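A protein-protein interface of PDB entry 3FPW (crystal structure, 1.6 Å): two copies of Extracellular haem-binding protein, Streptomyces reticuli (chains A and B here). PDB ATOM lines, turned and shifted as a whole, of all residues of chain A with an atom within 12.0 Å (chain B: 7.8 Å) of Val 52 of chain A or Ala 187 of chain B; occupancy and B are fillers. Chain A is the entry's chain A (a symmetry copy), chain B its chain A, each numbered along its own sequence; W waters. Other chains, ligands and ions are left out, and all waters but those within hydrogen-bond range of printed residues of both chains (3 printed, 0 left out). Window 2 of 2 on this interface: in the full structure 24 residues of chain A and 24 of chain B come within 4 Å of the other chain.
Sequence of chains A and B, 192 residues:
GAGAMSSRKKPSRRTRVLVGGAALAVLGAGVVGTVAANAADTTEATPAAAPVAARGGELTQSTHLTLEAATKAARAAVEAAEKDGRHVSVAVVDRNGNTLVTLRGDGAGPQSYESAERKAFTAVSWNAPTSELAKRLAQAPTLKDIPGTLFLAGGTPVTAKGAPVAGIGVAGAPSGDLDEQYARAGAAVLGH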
ATOM      1  N   PRO A  51     -27.755 -26.452   2.445  1.00  0.00           N
ATOM      2  CA  PRO A  51     -28.516 -26.459   1.189  1.00  0.00           C
ATOM      3  C   PRO A  51     -29.368 -25.228   1.009  1.00  0.00           C
ATOM      4  O   PRO A  51     -30.175 -24.867   1.857  1.00  0.00           O
ATOM      5  CB  PRO A  51     -29.382 -27.669   1.127  1.00  0.00           C
ATOM      6  N   VAL A  52     -29.200 -24.616  -0.149  1.00  0.00           N
ATOM      7  CA  VAL A  52     -30.188 -23.728  -0.665  1.00  0.00           C
ATOM      8  C   VAL A  52     -31.437 -24.551  -0.939  1.00  0.00           C
ATOM      9  O   VAL A  52     -31.358 -25.738  -1.305  1.00  0.00           O
ATOM     10  CB  VAL A  52     -29.660 -23.060  -1.946  1.00  0.00           C
ATOM     11  CG1 VAL A  52     -30.769 -22.308  -2.646  1.00  0.00           C
ATOM     12  CG2 VAL A  52     -28.526 -22.125  -1.588  1.00  0.00           C
ATOM     13  N   ALA A  53     -32.597 -23.938  -0.732  1.00  0.00           N
ATOM     14  CA  ALA A  53     -33.840 -24.572  -1.104  1.00  0.00           C
ATOM     15  C   ALA A  53     -34.393 -23.931  -2.375  1.00  0.00           C
ATOM     16  O   ALA A  53     -34.635 -22.727  -2.428  1.00  0.00           O
ATOM     17  CB  ALA A  53     -34.845 -24.469   0.031  1.00  0.00           C
ATOM     18  N   ALA A  54     -34.624 -24.734  -3.397  1.00  0.00           N
ATOM     19  CA  ALA A  54     -35.136 -24.182  -4.620  1.00  0.00           C
ATOM     20  C   ALA A  54     -36.645 -23.984  -4.521  1.00  0.00           C
ATOM     21  O   ALA A  54     -37.336 -24.594  -3.686  1.00  0.00           O
ATOM     22  CB  ALA A  54     -34.748 -25.029  -5.807  1.00  0.00           C
ATOM     23  N   ARG A  55     -37.133 -23.083  -5.363  1.00  0.00           N
ATOM     24  CA  ARG A  55     -38.515 -22.609  -5.353  1.00  0.00           C
ATOM     25  C   ARG A  55     -38.585 -21.761  -6.617  1.00  0.00           C
ATOM     26  O   ARG A  55     -37.800 -20.802  -6.763  1.00  0.00           O
ATOM     27  CB  ARG A  55     -38.762 -21.682  -4.149  1.00  0.00           C
ATOM     28  CG  ARG A  55     -39.102 -22.362  -2.832  1.00  0.00           C
ATOM     29  CD  ARG A  55     -40.615 -22.362  -2.578  1.00  0.00           C
ATOM     30  NE  ARG A  55     -41.338 -23.403  -3.312  1.00  0.00           N
ATOM     31  CZ  ARG A  55     -42.652 -23.605  -3.213  1.00  0.00           C
ATOM     32  NH1 ARG A  55     -43.382 -22.838  -2.415  1.00  0.00           N
ATOM     33  NH2 ARG A  55     -43.239 -24.567  -3.908  1.00  0.00           N
ATOM     34  N   GLY A  56     -39.509 -22.051  -7.522  1.00  0.00           N
ATOM     35  CA  GLY A  56     -40.597 -23.013  -7.348  1.00  0.00           C
ATOM     36  C   GLY A  56     -40.980 -23.145  -8.806  1.00  0.00           C
ATOM     37  O   GLY A  56     -41.261 -24.237  -9.306  1.00  0.00           O
ATOM     38  N   GLU A  58     -38.708 -22.923 -10.418  1.00  0.00           N
ATOM     39  CA  GLU A  58     -37.424 -23.600 -10.669  1.00  0.00           C
ATOM     40  C   GLU A  58     -37.543 -25.118 -10.549  1.00  0.00           C
ATOM     41  O   GLU A  58     -36.551 -25.830 -10.703  1.00  0.00           O
ATOM     42  CB  GLU A  58     -36.368 -23.108  -9.686  1.00  0.00           C
ATOM     43  CG  GLU A  58     -35.948 -21.660  -9.932  1.00  0.00           C
ATOM     44  CD  GLU A  58     -35.269 -21.046  -8.726  1.00  0.00           C
ATOM     45  OE1 GLU A  58     -35.522 -21.512  -7.593  1.00  0.00           O
ATOM     46  OE2 GLU A  58     -34.505 -20.069  -8.913  1.00  0.00           O
ATOM     47  N   LEU A  59     -38.739 -25.601 -10.232  1.00  0.00           N
ATOM     48  CA  LEU A  59     -38.935 -27.023  -9.940  1.00  0.00           C
ATOM     49  C   LEU A  59     -39.918 -27.635 -10.924  1.00  0.00           C
ATOM     50  O   LEU A  59     -40.814 -26.948 -11.439  1.00  0.00           O
ATOM     51  CB  LEU A  59     -39.451 -27.230  -8.512  1.00  0.00           C
ATOM     52  CG  LEU A  59     -38.536 -26.726  -7.380  1.00  0.00           C
ATOM     53  CD1 LEU A  59     -39.241 -26.863  -6.038  1.00  0.00           C
ATOM     54  CD2 LEU A  59     -37.244 -27.525  -7.367  1.00  0.00           C
ATOM     55  N   LEU B  65     -34.992 -29.945 -10.184  1.00  0.00           N
ATOM     56  CA  LEU B  65     -34.700 -28.677 -10.843  1.00  0.00           C
ATOM     57  C   LEU B  65     -35.070 -28.817 -12.311  1.00  0.00           C
ATOM     58  O   LEU B  65     -34.841 -29.870 -12.942  1.00  0.00           O
ATOM     59  CB  LEU B  65     -33.210 -28.324 -10.744  1.00  0.00           C
ATOM     60  CG  LEU B  65     -32.578 -28.082  -9.388  1.00  0.00           C
ATOM     61  CD1 LEU B  65     -31.135 -27.640  -9.577  1.00  0.00           C
ATOM     62  CD2 LEU B  65     -33.370 -27.032  -8.641  1.00  0.00           C
ATOM     63  N   LYS B  72     -29.030 -22.048 -14.865  1.00  0.00           N
ATOM     64  CA  LYS B  72     -28.808 -20.754 -14.195  1.00  0.00           C
ATOM     65  C   LYS B  72     -27.789 -20.926 -13.071  1.00  0.00           C
ATOM     66  O   LYS B  72     -26.878 -20.092 -12.927  1.00  0.00           O
ATOM     67  CB  LYS B  72     -30.156 -20.234 -13.664  1.00  0.00           C
ATOM     68  CG  LYS B  72     -30.104 -18.983 -12.794  1.00  0.00           C
ATOM     69  CD  LYS B  72     -31.506 -18.409 -12.545  1.00  0.00           C
ATOM     70  CE  LYS B  72     -32.302 -19.239 -11.533  1.00  0.00           C
ATOM     71  NZ  LYS B  72     -33.490 -18.489 -10.968  1.00  0.00           N
ATOM     72  N   ALA B  73     -27.941 -21.989 -12.280  1.00  0.00           N
ATOM     73  CA  ALA B  73     -27.052 -22.233 -11.150  1.00  0.00           C
ATOM     74  C   ALA B  73     -25.622 -22.540 -11.635  1.00  0.00           C
ATOM     75  O   ALA B  73     -24.628 -22.024 -11.106  1.00  0.00           O
ATOM     76  CB  ALA B  73     -27.591 -23.390 -10.281  1.00  0.00           C
ATOM     77  N   ALA B  74     -25.511 -23.396 -12.638  1.00  0.00           N
ATOM     78  CA  ALA B  74     -24.199 -23.750 -13.154  1.00  0.00           C
ATOM     79  C   ALA B  74     -23.493 -22.509 -13.662  1.00  0.00           C
ATOM     80  O   ALA B  74     -22.324 -22.285 -13.367  1.00  0.00           O
ATOM     81  CB  ALA B  74     -24.335 -24.781 -14.262  1.00  0.00           C
ATOM     82  N   ALA B  76     -23.959 -19.454 -12.820  1.00  0.00           N
ATOM     83  CA  ALA B  76     -23.604 -18.553 -11.713  1.00  0.00           C
ATOM     84  C   ALA B  76     -22.319 -18.997 -11.029  1.00  0.00           C
ATOM     85  O   ALA B  76     -21.521 -18.183 -10.593  1.00  0.00           O
ATOM     86  CB  ALA B  76     -24.745 -18.479 -10.717  1.00  0.00           C
ATOM     87  N   ALA B  77     -22.115 -20.296 -10.931  1.00  0.00           N
ATOM     88  CA  ALA B  77     -20.895 -20.810 -10.326  1.00  0.00           C
ATOM     89  C   ALA B  77     -19.713 -20.471 -11.222  1.00  0.00           C
ATOM     90  O   ALA B  77     -18.685 -20.012 -10.741  1.00  0.00           O
ATOM     91  CB  ALA B  77     -21.006 -22.315 -10.091  1.00  0.00           C
ATOM     92  N   ASN B 127     -26.983 -35.493   0.750  1.00  0.00           N
ATOM     93  CA  ASN B 127     -27.600 -34.226   1.110  1.00  0.00           C
ATOM     94  C   ASN B 127     -26.717 -33.413   2.056  1.00  0.00           C
ATOM     95  O   ASN B 127     -27.176 -32.899   3.093  1.00  0.00           O
ATOM     96  CB  ASN B 127     -28.994 -34.432   1.704  1.00  0.00           C
ATOM     97  CG  ASN B 127     -29.747 -33.143   1.837  1.00  0.00           C
ATOM     98  OD1 ASN B 127     -29.488 -32.187   1.102  1.00  0.00           O
ATOM     99  ND2 ASN B 127     -30.714 -33.104   2.763  1.00  0.00           N
ATOM    100  N   THR B 156     -22.134 -29.166  -3.326  1.00  0.00           N
ATOM    101  CA  THR B 156     -23.119 -28.707  -2.333  1.00  0.00           C
ATOM    102  C   THR B 156     -24.529 -29.096  -2.778  1.00  0.00           C
ATOM    103  O   THR B 156     -24.840 -29.024  -3.958  1.00  0.00           O
ATOM    104  CB  THR B 156     -22.992 -27.176  -2.066  1.00  0.00           C
ATOM    105  OG1 THR B 156     -23.679 -26.855  -0.851  1.00  0.00           O
ATOM    106  CG2 THR B 156     -23.548 -26.359  -3.193  1.00  0.00           C
ATOM    107  N   PRO B 157     -25.388 -29.497  -1.825  1.00  0.00           N
ATOM    108  CA  PRO B 157     -26.726 -29.925  -2.228  1.00  0.00           C
ATOM    109  C   PRO B 157     -27.737 -28.793  -2.352  1.00  0.00           C
ATOM    110  O   PRO B 157     -27.580 -27.706  -1.774  1.00  0.00           O
ATOM    111  CB  PRO B 157     -27.149 -30.859  -1.089  1.00  0.00           C
ATOM    112  CG  PRO B 157     -26.463 -30.270   0.116  1.00  0.00           C
ATOM    113  CD  PRO B 157     -25.114 -29.802  -0.407  1.00  0.00           C
ATOM    114  N   VAL B 158     -28.785 -29.082  -3.103  1.00  0.00           N
ATOM    115  CA  VAL B 158     -29.909 -28.175  -3.245  1.00  0.00           C
ATOM    116  C   VAL B 158     -31.129 -28.997  -2.922  1.00  0.00           C
ATOM    117  O   VAL B 158     -31.245 -30.157  -3.357  1.00  0.00           O
ATOM    118  CB  VAL B 158     -30.009 -27.633  -4.685  1.00  0.00           C
ATOM    119  CG1 VAL B 158     -31.315 -26.897  -4.895  1.00  0.00           C
ATOM    120  CG2 VAL B 158     -28.792 -26.718  -5.017  1.00  0.00           C
ATOM    121  N   THR B 159     -32.039 -28.427  -2.140  1.00  0.00           N
ATOM    122  CA  THR B 159     -33.202 -29.183  -1.725  1.00  0.00           C
ATOM    123  C   THR B 159     -34.490 -28.575  -2.226  1.00  0.00           C
ATOM    124  O   THR B 159     -34.514 -27.462  -2.742  1.00  0.00           O
ATOM    125  CB  THR B 159     -33.324 -29.266  -0.183  1.00  0.00           C
ATOM    126  OG1 THR B 159     -33.435 -27.938   0.343  1.00  0.00           O
ATOM    127  CG2 THR B 159     -32.108 -29.973   0.431  1.00  0.00           C
ATOM    128  N   ALA B 160     -35.558 -29.345  -2.072  1.00  0.00           N
ATOM    129  CA  ALA B 160     -36.922 -28.880  -2.286  1.00  0.00           C
ATOM    130  C   ALA B 160     -37.783 -29.663  -1.306  1.00  0.00           C
ATOM    131  O   ALA B 160     -37.682 -30.878  -1.230  1.00  0.00           O
ATOM    132  CB  ALA B 160     -37.357 -29.135  -3.738  1.00  0.00           C
ATOM    133  N   ALA B 163     -36.079 -32.185   0.936  1.00  0.00           N
ATOM    134  CA  ALA B 163     -35.425 -33.366   0.372  1.00  0.00           C
ATOM    135  C   ALA B 163     -34.401 -32.941  -0.672  1.00  0.00           C
ATOM    136  O   ALA B 163     -34.636 -31.995  -1.416  1.00  0.00           O
ATOM    137  CB  ALA B 163     -36.461 -34.293  -0.256  1.00  0.00           C
ATOM    138  N   PRO B 164     -33.272 -33.655  -0.760  1.00  0.00           N
ATOM    139  CA  PRO B 164     -32.285 -33.273  -1.790  1.00  0.00           C
ATOM    140  C   PRO B 164     -32.827 -33.486  -3.198  1.00  0.00           C
ATOM    141  O   PRO B 164     -33.428 -34.543  -3.461  1.00  0.00           O
ATOM    142  CB  PRO B 164     -31.094 -34.234  -1.510  1.00  0.00           C
ATOM    143  CG  PRO B 164     -31.697 -35.382  -0.763  1.00  0.00           C
ATOM    144  CD  PRO B 164     -32.823 -34.787   0.064  1.00  0.00           C
ATOM    145  N   VAL B 165     -32.638 -32.515  -4.095  1.00  0.00           N
ATOM    146  CA  VAL B 165     -33.068 -32.686  -5.497  1.00  0.00           C
ATOM    147  C   VAL B 165     -31.923 -32.579  -6.502  1.00  0.00           C
ATOM    148  O   VAL B 165     -32.023 -33.084  -7.621  1.00  0.00           O
ATOM    149  CB  VAL B 165     -34.223 -31.733  -5.906  1.00  0.00           C
ATOM    150  CG1 VAL B 165     -35.513 -32.056  -5.129  1.00  0.00           C
ATOM    151  CG2 VAL B 165     -33.803 -30.287  -5.695  1.00  0.00           C
ATOM    152  N   ALA B 166     -30.836 -31.927  -6.110  1.00  0.00           N
ATOM    153  CA  ALA B 166     -29.700 -31.793  -7.006  1.00  0.00           C
ATOM    154  C   ALA B 166     -28.432 -31.548  -6.197  1.00  0.00           C
ATOM    155  O   ALA B 166     -28.488 -31.155  -5.029  1.00  0.00           O
ATOM    156  CB  ALA B 166     -29.927 -30.641  -7.983  1.00  0.00           C
ATOM    157  N   GLY B 167     -27.299 -31.783  -6.831  1.00  0.00           N
ATOM    158  CA  GLY B 167     -26.017 -31.341  -6.270  1.00  0.00           C
ATOM    159  C   GLY B 167     -25.337 -30.474  -7.301  1.00  0.00           C
ATOM    160  O   GLY B 167     -25.445 -30.733  -8.498  1.00  0.00           O
ATOM    161  N   ILE B 168     -24.617 -29.445  -6.849  1.00  0.00           N
ATOM    162  CA  ILE B 168     -23.788 -28.633  -7.724  1.00  0.00           C
ATOM    163  C   ILE B 168     -22.338 -28.886  -7.327  1.00  0.00           C
ATOM    164  O   ILE B 168     -22.001 -28.795  -6.136  1.00  0.00           O
ATOM    165  CB  ILE B 168     -24.096 -27.146  -7.548  1.00  0.00           C
ATOM    166  CG1 ILE B 168     -25.561 -26.884  -7.886  1.00  0.00           C
ATOM    167  CG2 ILE B 168     -23.161 -26.328  -8.436  1.00  0.00           C
ATOM    168  CD1 ILE B 168     -26.035 -25.464  -7.560  1.00  0.00           C
ATOM    169  N   GLU B 180     -15.820 -24.973  -3.426  1.00  0.00           N
ATOM    170  CA  GLU B 180     -17.115 -25.034  -2.763  1.00  0.00           C
ATOM    171  C   GLU B 180     -17.742 -23.652  -2.585  1.00  0.00           C
ATOM    172  O   GLU B 180     -18.963 -23.524  -2.595  1.00  0.00           O
ATOM    173  CB  GLU B 180     -17.039 -25.814  -1.448  1.00  0.00           C
ATOM    174  CG  GLU B 180     -18.333 -26.529  -1.148  1.00  0.00           C
ATOM    175  CD  GLU B 180     -18.192 -27.487   0.013  1.00  0.00           C
ATOM    176  OE1 GLU B 180     -18.551 -27.104   1.147  1.00  0.00           O
ATOM    177  OE2 GLU B 180     -17.704 -28.609  -0.213  1.00  0.00           O
ATOM    178  N   GLN B 181     -16.908 -22.621  -2.425  1.00  0.00           N
ATOM    179  CA  GLN B 181     -17.393 -21.239  -2.478  1.00  0.00           C
ATOM    180  C   GLN B 181     -18.140 -20.985  -3.782  1.00  0.00           C
ATOM    181  O   GLN B 181     -19.230 -20.415  -3.785  1.00  0.00           O
ATOM    182  CB  GLN B 181     -16.217 -20.266  -2.357  1.00  0.00           C
ATOM    183  CG  GLN B 181     -16.565 -18.777  -2.368  1.00  0.00           C
ATOM    184  CD  GLN B 181     -15.334 -17.899  -2.104  1.00  0.00           C
ATOM    185  OE1 GLN B 181     -14.851 -17.203  -2.995  1.00  0.00           O
ATOM    186  NE2 GLN B 181     -14.815 -17.957  -0.886  1.00  0.00           N
ATOM    187  N   TYR B 182     -17.557 -21.398  -4.899  1.00  0.00           N
ATOM    188  CA  TYR B 182     -18.211 -21.129  -6.181  1.00  0.00           C
ATOM    189  C   TYR B 182     -19.461 -21.990  -6.372  1.00  0.00           C
ATOM    190  O   TYR B 182     -20.447 -21.541  -6.974  1.00  0.00           O
ATOM    191  CB  TYR B 182     -17.237 -21.351  -7.334  1.00  0.00           C
ATOM    192  CG  TYR B 182     -15.972 -20.529  -7.189  1.00  0.00           C
ATOM    193  CD1 TYR B 182     -16.035 -19.196  -6.812  1.00  0.00           C
ATOM    194  CD2 TYR B 182     -14.739 -21.073  -7.465  1.00  0.00           C
ATOM    195  CE1 TYR B 182     -14.893 -18.438  -6.679  1.00  0.00           C
ATOM    196  CE2 TYR B 182     -13.588 -20.334  -7.337  1.00  0.00           C
ATOM    197  CZ  TYR B 182     -13.673 -19.006  -6.947  1.00  0.00           C
ATOM    198  OH  TYR B 182     -12.530 -18.238  -6.818  1.00  0.00           O
ATOM    199  N   ALA B 183     -19.439 -23.212  -5.849  1.00  0.00           N
ATOM    200  CA  ALA B 183     -20.631 -24.064  -5.873  1.00  0.00           C
ATOM    201  C   ALA B 183     -21.772 -23.387  -5.105  1.00  0.00           C
ATOM    202  O   ALA B 183     -22.889 -23.340  -5.569  1.00  0.00           O
ATOM    203  CB  ALA B 183     -20.342 -25.461  -5.276  1.00  0.00           C
ATOM    204  N   ARG B 184     -21.467 -22.856  -3.922  1.00  0.00           N
ATOM    205  CA  ARG B 184     -22.466 -22.152  -3.141  1.00  0.00           C
ATOM    206  C   ARG B 184     -22.977 -20.912  -3.865  1.00  0.00           C
ATOM    207  O   ARG B 184     -24.147 -20.559  -3.728  1.00  0.00           O
ATOM    208  CB  ARG B 184     -21.903 -21.750  -1.772  1.00  0.00           C
ATOM    209  CG  ARG B 184     -21.717 -22.924  -0.800  1.00  0.00           C
ATOM    210  CD  ARG B 184     -21.466 -22.409   0.618  1.00  0.00           C
ATOM    211  NE  ARG B 184     -20.322 -21.505   0.688  1.00  0.00           N
ATOM    212  CZ  ARG B 184     -19.067 -21.910   0.881  1.00  0.00           C
ATOM    213  NH1 ARG B 184     -18.798 -23.195   1.030  1.00  0.00           N
ATOM    214  NH2 ARG B 184     -18.077 -21.025   0.946  1.00  0.00           N
ATOM    215  N   ALA B 185     -22.107 -20.229  -4.607  1.00  0.00           N
ATOM    216  CA  ALA B 185     -22.523 -19.070  -5.395  1.00  0.00           C
ATOM    217  C   ALA B 185     -23.512 -19.461  -6.486  1.00  0.00           C
ATOM    218  O   ALA B 185     -24.442 -18.716  -6.796  1.00  0.00           O
ATOM    219  CB  ALA B 185     -21.303 -18.381  -6.010  1.00  0.00           C
ATOM    220  N   GLY B 186     -23.307 -20.640  -7.072  1.00  0.00           N
ATOM    221  CA  GLY B 186     -24.266 -21.171  -8.033  1.00  0.00           C
ATOM    222  C   GLY B 186     -25.599 -21.522  -7.386  1.00  0.00           C
ATOM    223  O   GLY B 186     -26.657 -21.146  -7.881  1.00  0.00           O
ATOM    224  N   ALA B 187     -25.568 -22.222  -6.258  1.00  0.00           N
ATOM    225  CA  ALA B 187     -26.809 -22.545  -5.563  1.00  0.00           C
ATOM    226  C   ALA B 187     -27.576 -21.303  -5.123  1.00  0.00           C
ATOM    227  O   ALA B 187     -28.810 -21.305  -5.091  1.00  0.00           O
ATOM    228  CB  ALA B 187     -26.532 -23.410  -4.359  1.00  0.00           C
ATOM    229  N   ALA B 188     -26.833 -20.246  -4.798  1.00  0.00           N
ATOM    230  CA  ALA B 188     -27.413 -19.030  -4.211  1.00  0.00           C
ATOM    231  C   ALA B 188     -28.411 -18.327  -5.117  1.00  0.00           C
ATOM    232  O   ALA B 188     -29.227 -17.523  -4.632  1.00  0.00           O
ATOM    233  CB  ALA B 188     -26.299 -18.056  -3.817  1.00  0.00           C
ATOM    234  N   VAL B 189     -28.342 -18.591  -6.417  1.00  0.00           N
ATOM    235  CA  VAL B 189     -29.240 -17.924  -7.340  1.00  0.00           C
ATOM    236  C   VAL B 189     -30.571 -18.613  -7.446  1.00  0.00           C
ATOM    237  O   VAL B 189     -31.478 -18.091  -8.108  1.00  0.00           O
ATOM    238  CB  VAL B 189     -28.647 -17.755  -8.731  1.00  0.00           C
ATOM    239  CG1 VAL B 189     -27.318 -17.015  -8.640  1.00  0.00           C
ATOM    240  CG2 VAL B 189     -28.498 -19.113  -9.391  1.00  0.00           C
ATOM    241  N   LEU B 190     -30.703 -19.749  -6.772  1.00  0.00           N
ATOM    242  CA  LEU B 190     -31.958 -20.493  -6.769  1.00  0.00           C
ATOM    243  C   LEU B 190     -32.812 -20.094  -5.566  1.00  0.00           C
ATOM    244  O   LEU B 190     -32.313 -19.507  -4.603  1.00  0.00           O
ATOM    245  CB  LEU B 190     -31.682 -21.995  -6.719  1.00  0.00           C
ATOM    246  CG  LEU B 190     -30.842 -22.535  -7.879  1.00  0.00           C
ATOM    247  CD1 LEU B 190     -30.552 -24.010  -7.630  1.00  0.00           C
ATOM    248  CD2 LEU B 190     -31.588 -22.364  -9.176  1.00  0.00           C
HETATM  249  O   HOH W   1     -32.658 -26.265   2.524  1.00  0.00           O
HETATM  250  O   HOH W   2     -34.376 -17.637  -7.595  1.00  0.00           O
HETATM  251  O   HOH W   3     -26.229 -25.468  -1.385  1.00  0.00           O
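The side-chain amino group of Lys 72 of chain B lies within salt-bridge range of the side-chain carboxylate of Glu 58 of chain A (2.8 Å).
The backbone carbonyl oxygen of Val 52 of chain A sits at hydrogen-bond distance from the backbone NH of Thr 159 of chain B, at 2.9 Å.
The backbone carbonyl oxygen (O) of Thr 159 of chain B is in hydrogen-bond range of the backbone NH (N) of Ala 54 of chain A (2.8 Å).
The backbone carbonyl oxygen (O) of Val 158 of chain B lies within hydrogen-bond range of the backbone NH (N) of Val 165 of chain B, 2.8 Å away.
N of Val 158 of chain B sits at hydrogen-bond distance from O of Ala 166 of chain B.
The side-chain carboxylate (OE1) of Glu 58 of chain A is in hydrogen-bond range of the backbone NH (N) of Arg 55 of chain A (3.2 Å).
CA of Pro 51 of chain A touches O of Pro 157 of chain B, at 3.3 Å.
Thr 159 of chain B touches Pro 51 of chain A (CG2 to CB, 3.6 Å).
O of Pro 157 of chain B touches N of Val 52 of chain A (3.8 Å).
Val 52 of chain A touches Val 158 of chain B.
O of Ala 187 of chain B touches CG1 of Val 52 of chain A, 3.3 Å away.
CG1 of Val 52 of chain A touches O of Leu 190 of chain B (3.7 Å).
Thr 159 of chain B touches Ala 53 of chain A (O to CA, 3.4 Å).
Leu 65 of chain B touches Ala 54 of chain A.
O of Val 189 of chain B touches OE2 of Glu 58 of chain A, at 3.7 Å.
Ala 160 of chain B touches Leu 59 of chain A (CB to CD1, 3.7 Å).
Val 52 of chain A touches five residues of chain B.
Of the printed residues of chain B, Ala 53 of chain A touches Thr 159.
Printed residues of chain A within 4 Å of Leu 65 of chain B: Ala 54 and Glu 58.
Of the printed residues of chain A, Lys 72 of chain B touches Glu 58.
No residue of chain A comes within 4 Å of Ala 73 of chain B.
Ala 74 of chain B touches none of the printed residues of chain A.
No residue of chain A comes within 4 Å of Ala 76 of chain B.
No residue of chain A comes within 4 Å of Thr 156 of chain B.
Of the printed residues of chain A, Val 158 of chain B touches Val 52.
Thr 159 of chain B touches just these residues of chain A: Pro 51, Val 52, Ala 53 and Ala 54.
Of the printed residues of chain A, Ala 160 of chain B touches Leu 59 (3.7 Å).
Ile 168 of chain B touches none of the printed residues of chain A.
No residue of chain A comes within 4 Å of Ala 183 of chain B.
Of chain A, only Val 52 comes within 4 Å of Ala 187 of chain B.
Val 189 of chain B touches just one residue of chain A: Glu 58.
Leu 190 of chain B touches two residues of chain A.
The nearest printed residue of chain A that does not touch Leu 65 of chain B is Leu 59 of chain A (4.1 Å).
Among the printed residues, 15 pairs touch across the chains.
Among the printed residues, Asp or Glu carboxylates within 4 Å of a Lys or Arg side-chain nitrogen of the other chain: Glu 58 of chain A with Lys 72 of chain B.
No position is printed for both chains.
Of the 15 pairs that touch across the chains among the printed residues, none has its exchanged pair printed and touching as well.
Water W3 lies within hydrogen-bond range of O of Pro 157 of chain B (2.6 Å), OG1 of Thr 156 of chain B (3.0 Å) and N of Val 52 of chain A (3.3 Å).
Water W2 lies within hydrogen-bond range of the side-chain carboxylate (OE2) of Glu 58 of chain A and the backbone carbonyl oxygen (O) of Val 189 of chain B.
Water W1 bridges the side-chain hydroxyl (OG1) of Thr 159 of chain B (2.9 Å) and the backbone carbonyl oxygen (O) of Pro 51 of chain A (2.9 Å).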
